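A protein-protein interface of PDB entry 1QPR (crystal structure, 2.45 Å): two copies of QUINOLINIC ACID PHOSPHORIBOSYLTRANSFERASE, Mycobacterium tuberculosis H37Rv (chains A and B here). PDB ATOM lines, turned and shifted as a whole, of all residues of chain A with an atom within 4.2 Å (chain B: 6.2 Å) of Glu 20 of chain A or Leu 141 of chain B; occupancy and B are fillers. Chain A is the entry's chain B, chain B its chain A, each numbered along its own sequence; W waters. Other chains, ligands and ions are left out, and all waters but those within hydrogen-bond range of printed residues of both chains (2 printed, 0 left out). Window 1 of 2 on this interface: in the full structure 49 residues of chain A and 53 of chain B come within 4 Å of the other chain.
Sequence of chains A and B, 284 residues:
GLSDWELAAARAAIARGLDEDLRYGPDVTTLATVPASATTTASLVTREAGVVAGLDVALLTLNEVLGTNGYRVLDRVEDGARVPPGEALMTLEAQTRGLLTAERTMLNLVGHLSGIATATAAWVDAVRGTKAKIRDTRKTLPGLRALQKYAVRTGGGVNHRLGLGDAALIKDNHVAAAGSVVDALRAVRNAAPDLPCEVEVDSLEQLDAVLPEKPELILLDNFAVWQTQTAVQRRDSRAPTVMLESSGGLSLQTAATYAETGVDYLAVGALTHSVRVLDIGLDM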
ATOM      1  N   ARG A  16     -23.409 -27.898   8.187  1.00  0.00           N
ATOM      2  CA  ARG A  16     -21.969 -28.158   8.193  1.00  0.00           C
ATOM      3  C   ARG A  16     -21.280 -27.025   7.455  1.00  0.00           C
ATOM      4  O   ARG A  16     -20.226 -26.532   7.868  1.00  0.00           O
ATOM      5  CB  ARG A  16     -21.674 -29.500   7.531  1.00  0.00           C
ATOM      6  CG  ARG A  16     -22.317 -30.672   8.247  1.00  0.00           C
ATOM      7  CD  ARG A  16     -21.886 -32.022   7.708  1.00  0.00           C
ATOM      8  NE  ARG A  16     -22.429 -32.298   6.374  1.00  0.00           N
ATOM      9  CZ  ARG A  16     -23.366 -33.214   6.115  1.00  0.00           C
ATOM     10  NH1 ARG A  16     -23.872 -33.964   7.099  1.00  0.00           N
ATOM     11  NH2 ARG A  16     -23.844 -33.331   4.878  1.00  0.00           N
ATOM     12  N   GLY A  17     -21.901 -26.582   6.373  1.00  0.00           N
ATOM     13  CA  GLY A  17     -21.347 -25.493   5.590  1.00  0.00           C
ATOM     14  C   GLY A  17     -21.224 -24.226   6.409  1.00  0.00           C
ATOM     15  O   GLY A  17     -20.137 -23.628   6.475  1.00  0.00           O
ATOM     16  N   LEU A  18     -22.328 -23.802   7.035  1.00  0.00           N
ATOM     17  CA  LEU A  18     -22.298 -22.596   7.883  1.00  0.00           C
ATOM     18  C   LEU A  18     -21.310 -22.734   9.033  1.00  0.00           C
ATOM     19  O   LEU A  18     -20.625 -21.774   9.370  1.00  0.00           O
ATOM     20  CB  LEU A  18     -23.674 -22.273   8.443  1.00  0.00           C
ATOM     21  CG  LEU A  18     -24.696 -21.838   7.404  1.00  0.00           C
ATOM     22  CD1 LEU A  18     -25.998 -21.690   8.063  1.00  0.00           C
ATOM     23  CD2 LEU A  18     -24.277 -20.521   6.809  1.00  0.00           C
ATOM     24  N   ASP A  19     -21.220 -23.927   9.613  1.00  0.00           N
ATOM     25  CA  ASP A  19     -20.294 -24.130  10.696  1.00  0.00           C
ATOM     26  C   ASP A  19     -18.871 -23.969  10.213  1.00  0.00           C
ATOM     27  O   ASP A  19     -18.024 -23.475  10.944  1.00  0.00           O
ATOM     28  CB  ASP A  19     -20.497 -25.471  11.399  1.00  0.00           C
ATOM     29  CG  ASP A  19     -19.426 -25.723  12.498  1.00  0.00           C
ATOM     30  OD1 ASP A  19     -19.440 -25.008  13.549  1.00  0.00           O
ATOM     31  OD2 ASP A  19     -18.540 -26.611  12.297  1.00  0.00           O
ATOM     32  N   GLU A  20     -18.581 -24.405   8.997  1.00  0.00           N
ATOM     33  CA  GLU A  20     -17.220 -24.226   8.495  1.00  0.00           C
ATOM     34  C   GLU A  20     -16.885 -22.725   8.372  1.00  0.00           C
ATOM     35  O   GLU A  20     -15.770 -22.298   8.675  1.00  0.00           O
ATOM     36  CB  GLU A  20     -17.045 -24.932   7.154  1.00  0.00           C
ATOM     37  CG  GLU A  20     -17.034 -26.421   7.295  1.00  0.00           C
ATOM     38  CD  GLU A  20     -17.070 -27.164   5.959  1.00  0.00           C
ATOM     39  OE1 GLU A  20     -17.867 -26.800   5.061  1.00  0.00           O
ATOM     40  OE2 GLU A  20     -16.311 -28.153   5.832  1.00  0.00           O
ATOM     41  N   ASP A  21     -17.863 -21.943   7.925  1.00  0.00           N
ATOM     42  CA  ASP A  21     -17.722 -20.494   7.780  1.00  0.00           C
ATOM     43  C   ASP A  21     -17.618 -19.712   9.099  1.00  0.00           C
ATOM     44  O   ASP A  21     -16.788 -18.809   9.244  1.00  0.00           O
ATOM     45  CB  ASP A  21     -18.921 -19.953   7.005  1.00  0.00           C
ATOM     46  CG  ASP A  21     -18.577 -19.596   5.608  1.00  0.00           C
ATOM     47  OD1 ASP A  21     -17.397 -19.702   5.212  1.00  0.00           O
ATOM     48  OD2 ASP A  21     -19.514 -19.223   4.880  1.00  0.00           O
ATOM     49  N   LEU A  22     -18.446 -20.100  10.061  1.00  0.00           N
ATOM     50  CA  LEU A  22     -18.523 -19.421  11.334  1.00  0.00           C
ATOM     51  C   LEU A  22     -17.664 -19.888  12.475  1.00  0.00           C
ATOM     52  O   LEU A  22     -17.534 -19.173  13.455  1.00  0.00           O
ATOM     53  CB  LEU A  22     -19.977 -19.356  11.781  1.00  0.00           C
ATOM     54  CG  LEU A  22     -20.825 -18.600  10.750  1.00  0.00           C
ATOM     55  CD1 LEU A  22     -22.316 -18.832  10.959  1.00  0.00           C
ATOM     56  CD2 LEU A  22     -20.505 -17.148  10.795  1.00  0.00           C
ATOM     57  N   ARG A  23     -16.982 -21.005  12.345  1.00  0.00           N
ATOM     58  CA  ARG A  23     -16.197 -21.466  13.471  1.00  0.00           C
ATOM     59  C   ARG A  23     -14.987 -20.630  13.886  1.00  0.00           C
ATOM     60  O   ARG A  23     -14.389 -20.878  14.944  1.00  0.00           O
ATOM     61  CB  ARG A  23     -15.808 -22.938  13.303  1.00  0.00           C
ATOM     62  CG  ARG A  23     -14.734 -23.249  12.278  1.00  0.00           C
ATOM     63  CD  ARG A  23     -14.587 -24.745  12.125  1.00  0.00           C
ATOM     64  NE  ARG A  23     -14.044 -25.365  13.329  1.00  0.00           N
ATOM     65  CZ  ARG A  23     -12.756 -25.338  13.680  1.00  0.00           C
ATOM     66  NH1 ARG A  23     -11.862 -24.720  12.917  1.00  0.00           N
ATOM     67  NH2 ARG A  23     -12.352 -25.937  14.793  1.00  0.00           N
ATOM     68  N   TYR A  24     -14.605 -19.649  13.079  1.00  0.00           N
ATOM     69  CA  TYR A  24     -13.448 -18.826  13.430  1.00  0.00           C
ATOM     70  C   TYR A  24     -13.854 -17.467  13.971  1.00  0.00           C
ATOM     71  O   TYR A  24     -13.003 -16.627  14.250  1.00  0.00           O
ATOM     72  CB  TYR A  24     -12.533 -18.643  12.225  1.00  0.00           C
ATOM     73  CG  TYR A  24     -12.118 -19.945  11.666  1.00  0.00           C
ATOM     74  CD1 TYR A  24     -11.057 -20.644  12.225  1.00  0.00           C
ATOM     75  CD2 TYR A  24     -12.850 -20.542  10.654  1.00  0.00           C
ATOM     76  CE1 TYR A  24     -10.744 -21.918  11.795  1.00  0.00           C
ATOM     77  CE2 TYR A  24     -12.552 -21.820  10.213  1.00  0.00           C
ATOM     78  CZ  TYR A  24     -11.501 -22.504  10.790  1.00  0.00           C
ATOM     79  OH  TYR A  24     -11.220 -23.786  10.381  1.00  0.00           O
ATOM     80  N   HIS A 112     -23.005 -26.723  -7.233  1.00  0.00           N
ATOM     81  CA  HIS A 112     -22.621 -28.115  -7.321  1.00  0.00           C
ATOM     82  C   HIS A 112     -23.799 -28.869  -7.892  1.00  0.00           C
ATOM     83  O   HIS A 112     -23.701 -29.407  -8.982  1.00  0.00           O
ATOM     84  CB  HIS A 112     -22.221 -28.662  -5.955  1.00  0.00           C
ATOM     85  CG  HIS A 112     -21.750 -30.083  -5.981  1.00  0.00           C
ATOM     86  ND1 HIS A 112     -20.473 -30.441  -6.347  1.00  0.00           N
ATOM     87  CD2 HIS A 112     -22.399 -31.248  -5.735  1.00  0.00           C
ATOM     88  CE1 HIS A 112     -20.353 -31.758  -6.343  1.00  0.00           C
ATOM     89  NE2 HIS A 112     -21.508 -32.273  -5.973  1.00  0.00           N
ATOM     90  N   TRP B   5      -7.679 -31.040  13.652  1.00  0.00           N
ATOM     91  CA  TRP B   5      -8.987 -30.673  13.133  1.00  0.00           C
ATOM     92  C   TRP B   5      -9.249 -31.325  11.804  1.00  0.00           C
ATOM     93  O   TRP B   5     -10.390 -31.652  11.491  1.00  0.00           O
ATOM     94  CB  TRP B   5      -9.225 -29.145  13.181  1.00  0.00           C
ATOM     95  CG  TRP B   5      -9.196 -28.373  11.893  1.00  0.00           C
ATOM     96  CD1 TRP B   5      -8.085 -27.904  11.243  1.00  0.00           C
ATOM     97  CD2 TRP B   5     -10.335 -27.881  11.142  1.00  0.00           C
ATOM     98  NE1 TRP B   5      -8.455 -27.145  10.143  1.00  0.00           N
ATOM     99  CE2 TRP B   5      -9.825 -27.115  10.058  1.00  0.00           C
ATOM    100  CE3 TRP B   5     -11.732 -28.011  11.282  1.00  0.00           C
ATOM    101  CZ2 TRP B   5     -10.662 -26.477   9.118  1.00  0.00           C
ATOM    102  CZ3 TRP B   5     -12.569 -27.372  10.342  1.00  0.00           C
ATOM    103  CH2 TRP B   5     -12.024 -26.615   9.275  1.00  0.00           C
ATOM    104  N   HIS B 112     -11.037 -38.139  -4.447  1.00  0.00           N
ATOM    105  CA  HIS B 112     -11.389 -36.723  -4.440  1.00  0.00           C
ATOM    106  C   HIS B 112     -10.197 -35.893  -4.025  1.00  0.00           C
ATOM    107  O   HIS B 112      -9.750 -35.021  -4.761  1.00  0.00           O
ATOM    108  CB  HIS B 112     -12.570 -36.468  -3.506  1.00  0.00           C
ATOM    109  CG  HIS B 112     -13.065 -35.056  -3.521  1.00  0.00           C
ATOM    110  ND1 HIS B 112     -13.865 -34.555  -4.524  1.00  0.00           N
ATOM    111  CD2 HIS B 112     -12.835 -34.027  -2.675  1.00  0.00           C
ATOM    112  CE1 HIS B 112     -14.100 -33.278  -4.300  1.00  0.00           C
ATOM    113  NE2 HIS B 112     -13.485 -32.932  -3.185  1.00  0.00           N
ATOM    114  N   ARG B 138     -13.143 -20.153  -0.771  1.00  0.00           N
ATOM    115  CA  ARG B 138     -14.157 -20.701   0.101  1.00  0.00           C
ATOM    116  C   ARG B 138     -15.172 -21.416  -0.757  1.00  0.00           C
ATOM    117  O   ARG B 138     -16.229 -21.791  -0.301  1.00  0.00           O
ATOM    118  CB  ARG B 138     -14.824 -19.620   0.934  1.00  0.00           C
ATOM    119  CG  ARG B 138     -14.017 -19.170   2.172  1.00  0.00           C
ATOM    120  CD  ARG B 138     -14.934 -18.392   3.124  1.00  0.00           C
ATOM    121  NE  ARG B 138     -15.529 -17.255   2.435  1.00  0.00           N
ATOM    122  CZ  ARG B 138     -16.827 -16.978   2.390  1.00  0.00           C
ATOM    123  NH1 ARG B 138     -17.716 -17.722   3.010  1.00  0.00           N
ATOM    124  NH2 ARG B 138     -17.253 -16.025   1.609  1.00  0.00           N
ATOM    125  N   LYS B 139     -14.840 -21.616  -2.019  1.00  0.00           N
ATOM    126  CA  LYS B 139     -15.732 -22.307  -2.890  1.00  0.00           C
ATOM    127  C   LYS B 139     -15.418 -23.777  -2.721  1.00  0.00           C
ATOM    128  O   LYS B 139     -14.925 -24.423  -3.638  1.00  0.00           O
ATOM    129  CB  LYS B 139     -15.512 -21.855  -4.312  1.00  0.00           C
ATOM    130  CG  LYS B 139     -15.670 -20.375  -4.519  1.00  0.00           C
ATOM    131  CD  LYS B 139     -15.423 -20.052  -5.959  1.00  0.00           C
ATOM    132  CE  LYS B 139     -15.785 -18.634  -6.290  1.00  0.00           C
ATOM    133  NZ  LYS B 139     -16.812 -18.567  -7.413  1.00  0.00           N
ATOM    134  N   THR B 140     -15.703 -24.273  -1.519  1.00  0.00           N
ATOM    135  CA  THR B 140     -15.485 -25.657  -1.094  1.00  0.00           C
ATOM    136  C   THR B 140     -16.822 -26.402  -0.924  1.00  0.00           C
ATOM    137  O   THR B 140     -17.883 -25.796  -0.911  1.00  0.00           O
ATOM    138  CB  THR B 140     -14.728 -25.664   0.238  1.00  0.00           C
ATOM    139  OG1 THR B 140     -15.356 -24.755   1.150  1.00  0.00           O
ATOM    140  CG2 THR B 140     -13.310 -25.235   0.043  1.00  0.00           C
ATOM    141  N   LEU B 141     -16.801 -27.721  -0.821  1.00  0.00           N
ATOM    142  CA  LEU B 141     -18.060 -28.467  -0.645  1.00  0.00           C
ATOM    143  C   LEU B 141     -18.340 -28.549   0.844  1.00  0.00           C
ATOM    144  O   LEU B 141     -17.414 -28.710   1.651  1.00  0.00           O
ATOM    145  CB  LEU B 141     -17.989 -29.891  -1.244  1.00  0.00           C
ATOM    146  CG  LEU B 141     -18.339 -30.156  -2.716  1.00  0.00           C
ATOM    147  CD1 LEU B 141     -19.493 -29.248  -3.123  1.00  0.00           C
ATOM    148  CD2 LEU B 141     -17.158 -29.910  -3.629  1.00  0.00           C
ATOM    149  N   PRO B 142     -19.610 -28.390   1.229  1.00  0.00           N
ATOM    150  CA  PRO B 142     -20.029 -28.442   2.633  1.00  0.00           C
ATOM    151  C   PRO B 142     -19.672 -29.740   3.343  1.00  0.00           C
ATOM    152  O   PRO B 142     -20.124 -30.817   2.966  1.00  0.00           O
ATOM    153  CB  PRO B 142     -21.553 -28.227   2.561  1.00  0.00           C
ATOM    154  CG  PRO B 142     -21.914 -28.663   1.165  1.00  0.00           C
ATOM    155  CD  PRO B 142     -20.762 -28.132   0.343  1.00  0.00           C
ATOM    156  N   GLY B 143     -18.892 -29.608   4.410  1.00  0.00           N
ATOM    157  CA  GLY B 143     -18.463 -30.750   5.187  1.00  0.00           C
ATOM    158  C   GLY B 143     -17.098 -31.220   4.770  1.00  0.00           C
ATOM    159  O   GLY B 143     -16.504 -32.049   5.443  1.00  0.00           O
ATOM    160  N   LEU B 144     -16.550 -30.640   3.707  1.00  0.00           N
ATOM    161  CA  LEU B 144     -15.258 -31.079   3.210  1.00  0.00           C
ATOM    162  C   LEU B 144     -14.201 -30.013   3.110  1.00  0.00           C
ATOM    163  O   LEU B 144     -13.097 -30.269   2.608  1.00  0.00           O
ATOM    164  CB  LEU B 144     -15.432 -31.771   1.851  1.00  0.00           C
ATOM    165  CG  LEU B 144     -16.280 -33.047   1.846  1.00  0.00           C
ATOM    166  CD1 LEU B 144     -16.684 -33.449   0.439  1.00  0.00           C
ATOM    167  CD2 LEU B 144     -15.500 -34.159   2.492  1.00  0.00           C
ATOM    168  N   ARG B 145     -14.472 -28.840   3.653  1.00  0.00           N
ATOM    169  CA  ARG B 145     -13.486 -27.775   3.570  1.00  0.00           C
ATOM    170  C   ARG B 145     -12.092 -28.107   4.111  1.00  0.00           C
ATOM    171  O   ARG B 145     -11.080 -27.890   3.434  1.00  0.00           O
ATOM    172  CB  ARG B 145     -14.033 -26.464   4.191  1.00  0.00           C
ATOM    173  CG  ARG B 145     -12.971 -25.384   4.359  1.00  0.00           C
ATOM    174  CD  ARG B 145     -13.488 -23.958   4.487  1.00  0.00           C
ATOM    175  NE  ARG B 145     -14.539 -23.623   3.537  1.00  0.00           N
ATOM    176  CZ  ARG B 145     -15.387 -22.600   3.707  1.00  0.00           C
ATOM    177  NH1 ARG B 145     -15.275 -21.821   4.789  1.00  0.00           N
ATOM    178  NH2 ARG B 145     -16.394 -22.394   2.843  1.00  0.00           N
ATOM    179  N   ALA B 146     -12.025 -28.707   5.297  1.00  0.00           N
ATOM    180  CA  ALA B 146     -10.720 -28.981   5.906  1.00  0.00           C
ATOM    181  C   ALA B 146      -9.948 -29.949   5.074  1.00  0.00           C
ATOM    182  O   ALA B 146      -8.745 -29.770   4.858  1.00  0.00           O
ATOM    183  CB  ALA B 146     -10.858 -29.495   7.342  1.00  0.00           C
ATOM    184  N   GLN B 148     -10.428 -30.581   1.724  1.00  0.00           N
ATOM    185  CA  GLN B 148     -10.093 -30.007   0.422  1.00  0.00           C
ATOM    186  C   GLN B 148      -8.944 -29.036   0.566  1.00  0.00           C
ATOM    187  O   GLN B 148      -8.024 -28.990  -0.271  1.00  0.00           O
ATOM    188  CB  GLN B 148     -11.292 -29.311  -0.187  1.00  0.00           C
ATOM    189  CG  GLN B 148     -12.410 -30.256  -0.446  1.00  0.00           C
ATOM    190  CD  GLN B 148     -13.468 -29.590  -1.209  1.00  0.00           C
ATOM    191  OE1 GLN B 148     -13.931 -30.091  -2.232  1.00  0.00           O
ATOM    192  NE2 GLN B 148     -13.856 -28.431  -0.751  1.00  0.00           N
ATOM    193  N   LEU B 162      -9.841 -19.793   5.996  1.00  0.00           N
ATOM    194  CA  LEU B 162     -10.636 -20.979   6.237  1.00  0.00           C
ATOM    195  C   LEU B 162     -12.092 -20.670   6.478  1.00  0.00           C
ATOM    196  O   LEU B 162     -12.955 -21.522   6.279  1.00  0.00           O
ATOM    197  CB  LEU B 162     -10.049 -21.765   7.415  1.00  0.00           C
ATOM    198  CG  LEU B 162      -8.563 -22.175   7.320  1.00  0.00           C
ATOM    199  CD1 LEU B 162      -8.151 -22.803   8.621  1.00  0.00           C
ATOM    200  CD2 LEU B 162      -8.308 -23.165   6.203  1.00  0.00           C
ATOM    201  N   GLY B 163     -12.375 -19.439   6.870  1.00  0.00           N
ATOM    202  CA  GLY B 163     -13.733 -19.075   7.134  1.00  0.00           C
ATOM    203  C   GLY B 163     -13.943 -17.607   6.984  1.00  0.00           C
ATOM    204  O   GLY B 163     -13.114 -16.918   6.398  1.00  0.00           O
ATOM    205  N   LEU B 164     -15.031 -17.129   7.574  1.00  0.00           N
ATOM    206  CA  LEU B 164     -15.442 -15.728   7.521  1.00  0.00           C
ATOM    207  C   LEU B 164     -14.799 -14.800   8.590  1.00  0.00           C
ATOM    208  O   LEU B 164     -14.581 -13.592   8.334  1.00  0.00           O
ATOM    209  CB  LEU B 164     -16.971 -15.670   7.618  1.00  0.00           C
ATOM    210  CG  LEU B 164     -17.840 -15.202   6.460  1.00  0.00           C
ATOM    211  CD1 LEU B 164     -17.111 -15.126   5.148  1.00  0.00           C
ATOM    212  CD2 LEU B 164     -19.040 -16.081   6.371  1.00  0.00           C
ATOM    213  N   THR B 272     -11.180 -26.406  -6.036  1.00  0.00           N
ATOM    214  CA  THR B 272     -12.020 -27.091  -5.053  1.00  0.00           C
ATOM    215  C   THR B 272     -13.488 -27.239  -5.445  1.00  0.00           C
ATOM    216  O   THR B 272     -14.222 -28.048  -4.858  1.00  0.00           O
ATOM    217  CB  THR B 272     -11.926 -26.386  -3.666  1.00  0.00           C
ATOM    218  OG1 THR B 272     -12.291 -24.999  -3.780  1.00  0.00           O
ATOM    219  CG2 THR B 272     -10.530 -26.441  -3.143  1.00  0.00           C
ATOM    220  N   HIS B 273     -13.938 -26.473  -6.436  1.00  0.00           N
ATOM    221  CA  HIS B 273     -15.330 -26.597  -6.849  1.00  0.00           C
ATOM    222  C   HIS B 273     -15.585 -27.368  -8.156  1.00  0.00           C
ATOM    223  O   HIS B 273     -16.718 -27.670  -8.481  1.00  0.00           O
ATOM    224  CB  HIS B 273     -16.017 -25.239  -6.884  1.00  0.00           C
ATOM    225  CG  HIS B 273     -15.497 -24.288  -7.928  1.00  0.00           C
ATOM    226  ND1 HIS B 273     -15.568 -24.539  -9.284  1.00  0.00           N
ATOM    227  CD2 HIS B 273     -14.966 -23.044  -7.812  1.00  0.00           C
ATOM    228  CE1 HIS B 273     -15.106 -23.499  -9.953  1.00  0.00           C
ATOM    229  NE2 HIS B 273     -14.733 -22.578  -9.083  1.00  0.00           N
ATOM    230  N   VAL B 275     -13.614 -30.387  -9.268  1.00  0.00           N
ATOM    231  CA  VAL B 275     -12.550 -31.383  -9.237  1.00  0.00           C
ATOM    232  C   VAL B 275     -12.882 -32.668 -10.017  1.00  0.00           C
ATOM    233  O   VAL B 275     -14.036 -33.151  -9.990  1.00  0.00           O
ATOM    234  CB  VAL B 275     -12.047 -31.722  -7.762  1.00  0.00           C
ATOM    235  CG1 VAL B 275     -12.671 -30.831  -6.739  1.00  0.00           C
ATOM    236  CG2 VAL B 275     -12.266 -33.171  -7.410  1.00  0.00           C
HETATM  237  O   HOH W   1     -17.363 -26.070   2.480  1.00  0.00           O
HETATM  238  O   HOH W   2     -19.113 -27.957  -7.426  1.00  0.00           O
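Position printed for both chains: 112.
Of the 15 pairs that touch across the chains among the printed residues, none has its exchanged pair printed and touching as well.
Glu 20 of chain A touches just these residues of chain B: Leu 141 (3.9 Å), Pro 142 (3.6 Å), Gly 143 (3.1 Å), Leu 144 (3.3 Å), Arg 145 (2.9 Å) and Leu 162 (3.8 Å).
Printed residues of chain B within 4 Å of Asp 21 of chain A: Arg 138, Arg 145, Gly 163 and Leu 164.
Leu 141 of chain B touches just these residues of chain A: Glu 20 and His 112.
Printed residues of chain A within 4 Å of Pro 142 of chain B: Glu 20.
Thr 272 of chain B touches none of the printed residues of chain A.
O of Arg 138 of chain B sits at hydrogen-bond distance from OG1 of Thr 140 of chain B (3.4 Å).
O of Arg 138 of chain B is in hydrogen-bond range of NH2 of Arg 145 of chain B, at 3.2 Å.
The side-chain hydroxyl (OG1) of Thr 140 of chain B lies within hydrogen-bond range of the guanidinium group (NE) of Arg 145 of chain B (2.8 Å).
The side-chain amide nitrogen (NE2) of Gln 148 of chain B sits close to the backbone NH (N) of Leu 141 of chain B.
The guanidinium group of Arg 145 of chain B lies within hydrogen-bond range of the backbone carbonyl oxygen of Leu 162 of chain B (2.8 Å).
The side-chain hydroxyl (OH) of Tyr 24 of chain A lies within hydrogen-bond range of the guanidinium group (NH1) of Arg 23 of chain A (2.8 Å).
Among the printed residues, pairs that only touch across the chains: Tyr 24 of chain A with Trp 5 of chain B (3.0 Å), His 112 of chain A with Leu 141 of chain B (3.6 Å), Glu 20 of chain A with Pro 142 of chain B (3.6 Å), Tyr 24 of chain A with Leu 162 of chain B (3.7 Å), Arg 23 of chain A with Trp 5 of chain B (3.7 Å), Asp 21 of chain A with Gly 163 of chain B (3.7 Å), Glu 20 of chain A with Leu 162 of chain B (3.8 Å), Tyr 24 of chain A with Gly 163 of chain B (3.9 Å) and Glu 20 of chain A with Leu 141 of chain B (3.9 Å).
Water W2 lies within hydrogen-bond range of O of His 273 of chain B (2.6 Å) and ND1 of His 112 of chain A (3.0 Å).
Water W1 lies within hydrogen-bond range of the side-chain carboxylate (OE1) of Glu 20 of chain A, the side-chain hydroxyl (OG1) of Thr 140 of chain B and the backbone carbonyl oxygen (O) of Leu 141 of chain B.
Hydrophobic or aromatic side chains of chain A within 4 Å of the printed part of chain B: Tyr 24 and His 112.
Among the printed residues, Asp or Glu carboxylates within 4 Å of a Lys or Arg side-chain nitrogen of the other chain: Asp 21 of chain A with Arg 138 of chain B (3.0 Å) and Asp 21 of chain A with Arg 145 of chain B (3.0 Å).
NH1 of Arg 138 of chain B is in salt-bridge range of OD1 of Asp 21 of chain A (3.0 Å).
N of Gly 143 of chain B sits at hydrogen-bond distance from OE1 of Glu 20 of chain A (3.1 Å).
The side-chain carboxylate (OE2) of Glu 20 of chain A lies within hydrogen-bond range of the backbone NH (N) of Leu 144 of chain B.
The backbone NH of Arg 145 of chain B sits at hydrogen-bond distance from the side-chain carboxylate of Glu 20 of chain A (2.9 Å).
The guanidinium group (NH1) of Arg 145 of chain B is in salt-bridge range of the side-chain carboxylate (OD1) of Asp 21 of chain A (3.0 Å).
The backbone carbonyl oxygen (O) of Asp 21 of chain A sits at hydrogen-bond distance from the backbone NH (N) of Leu 164 of chain B.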
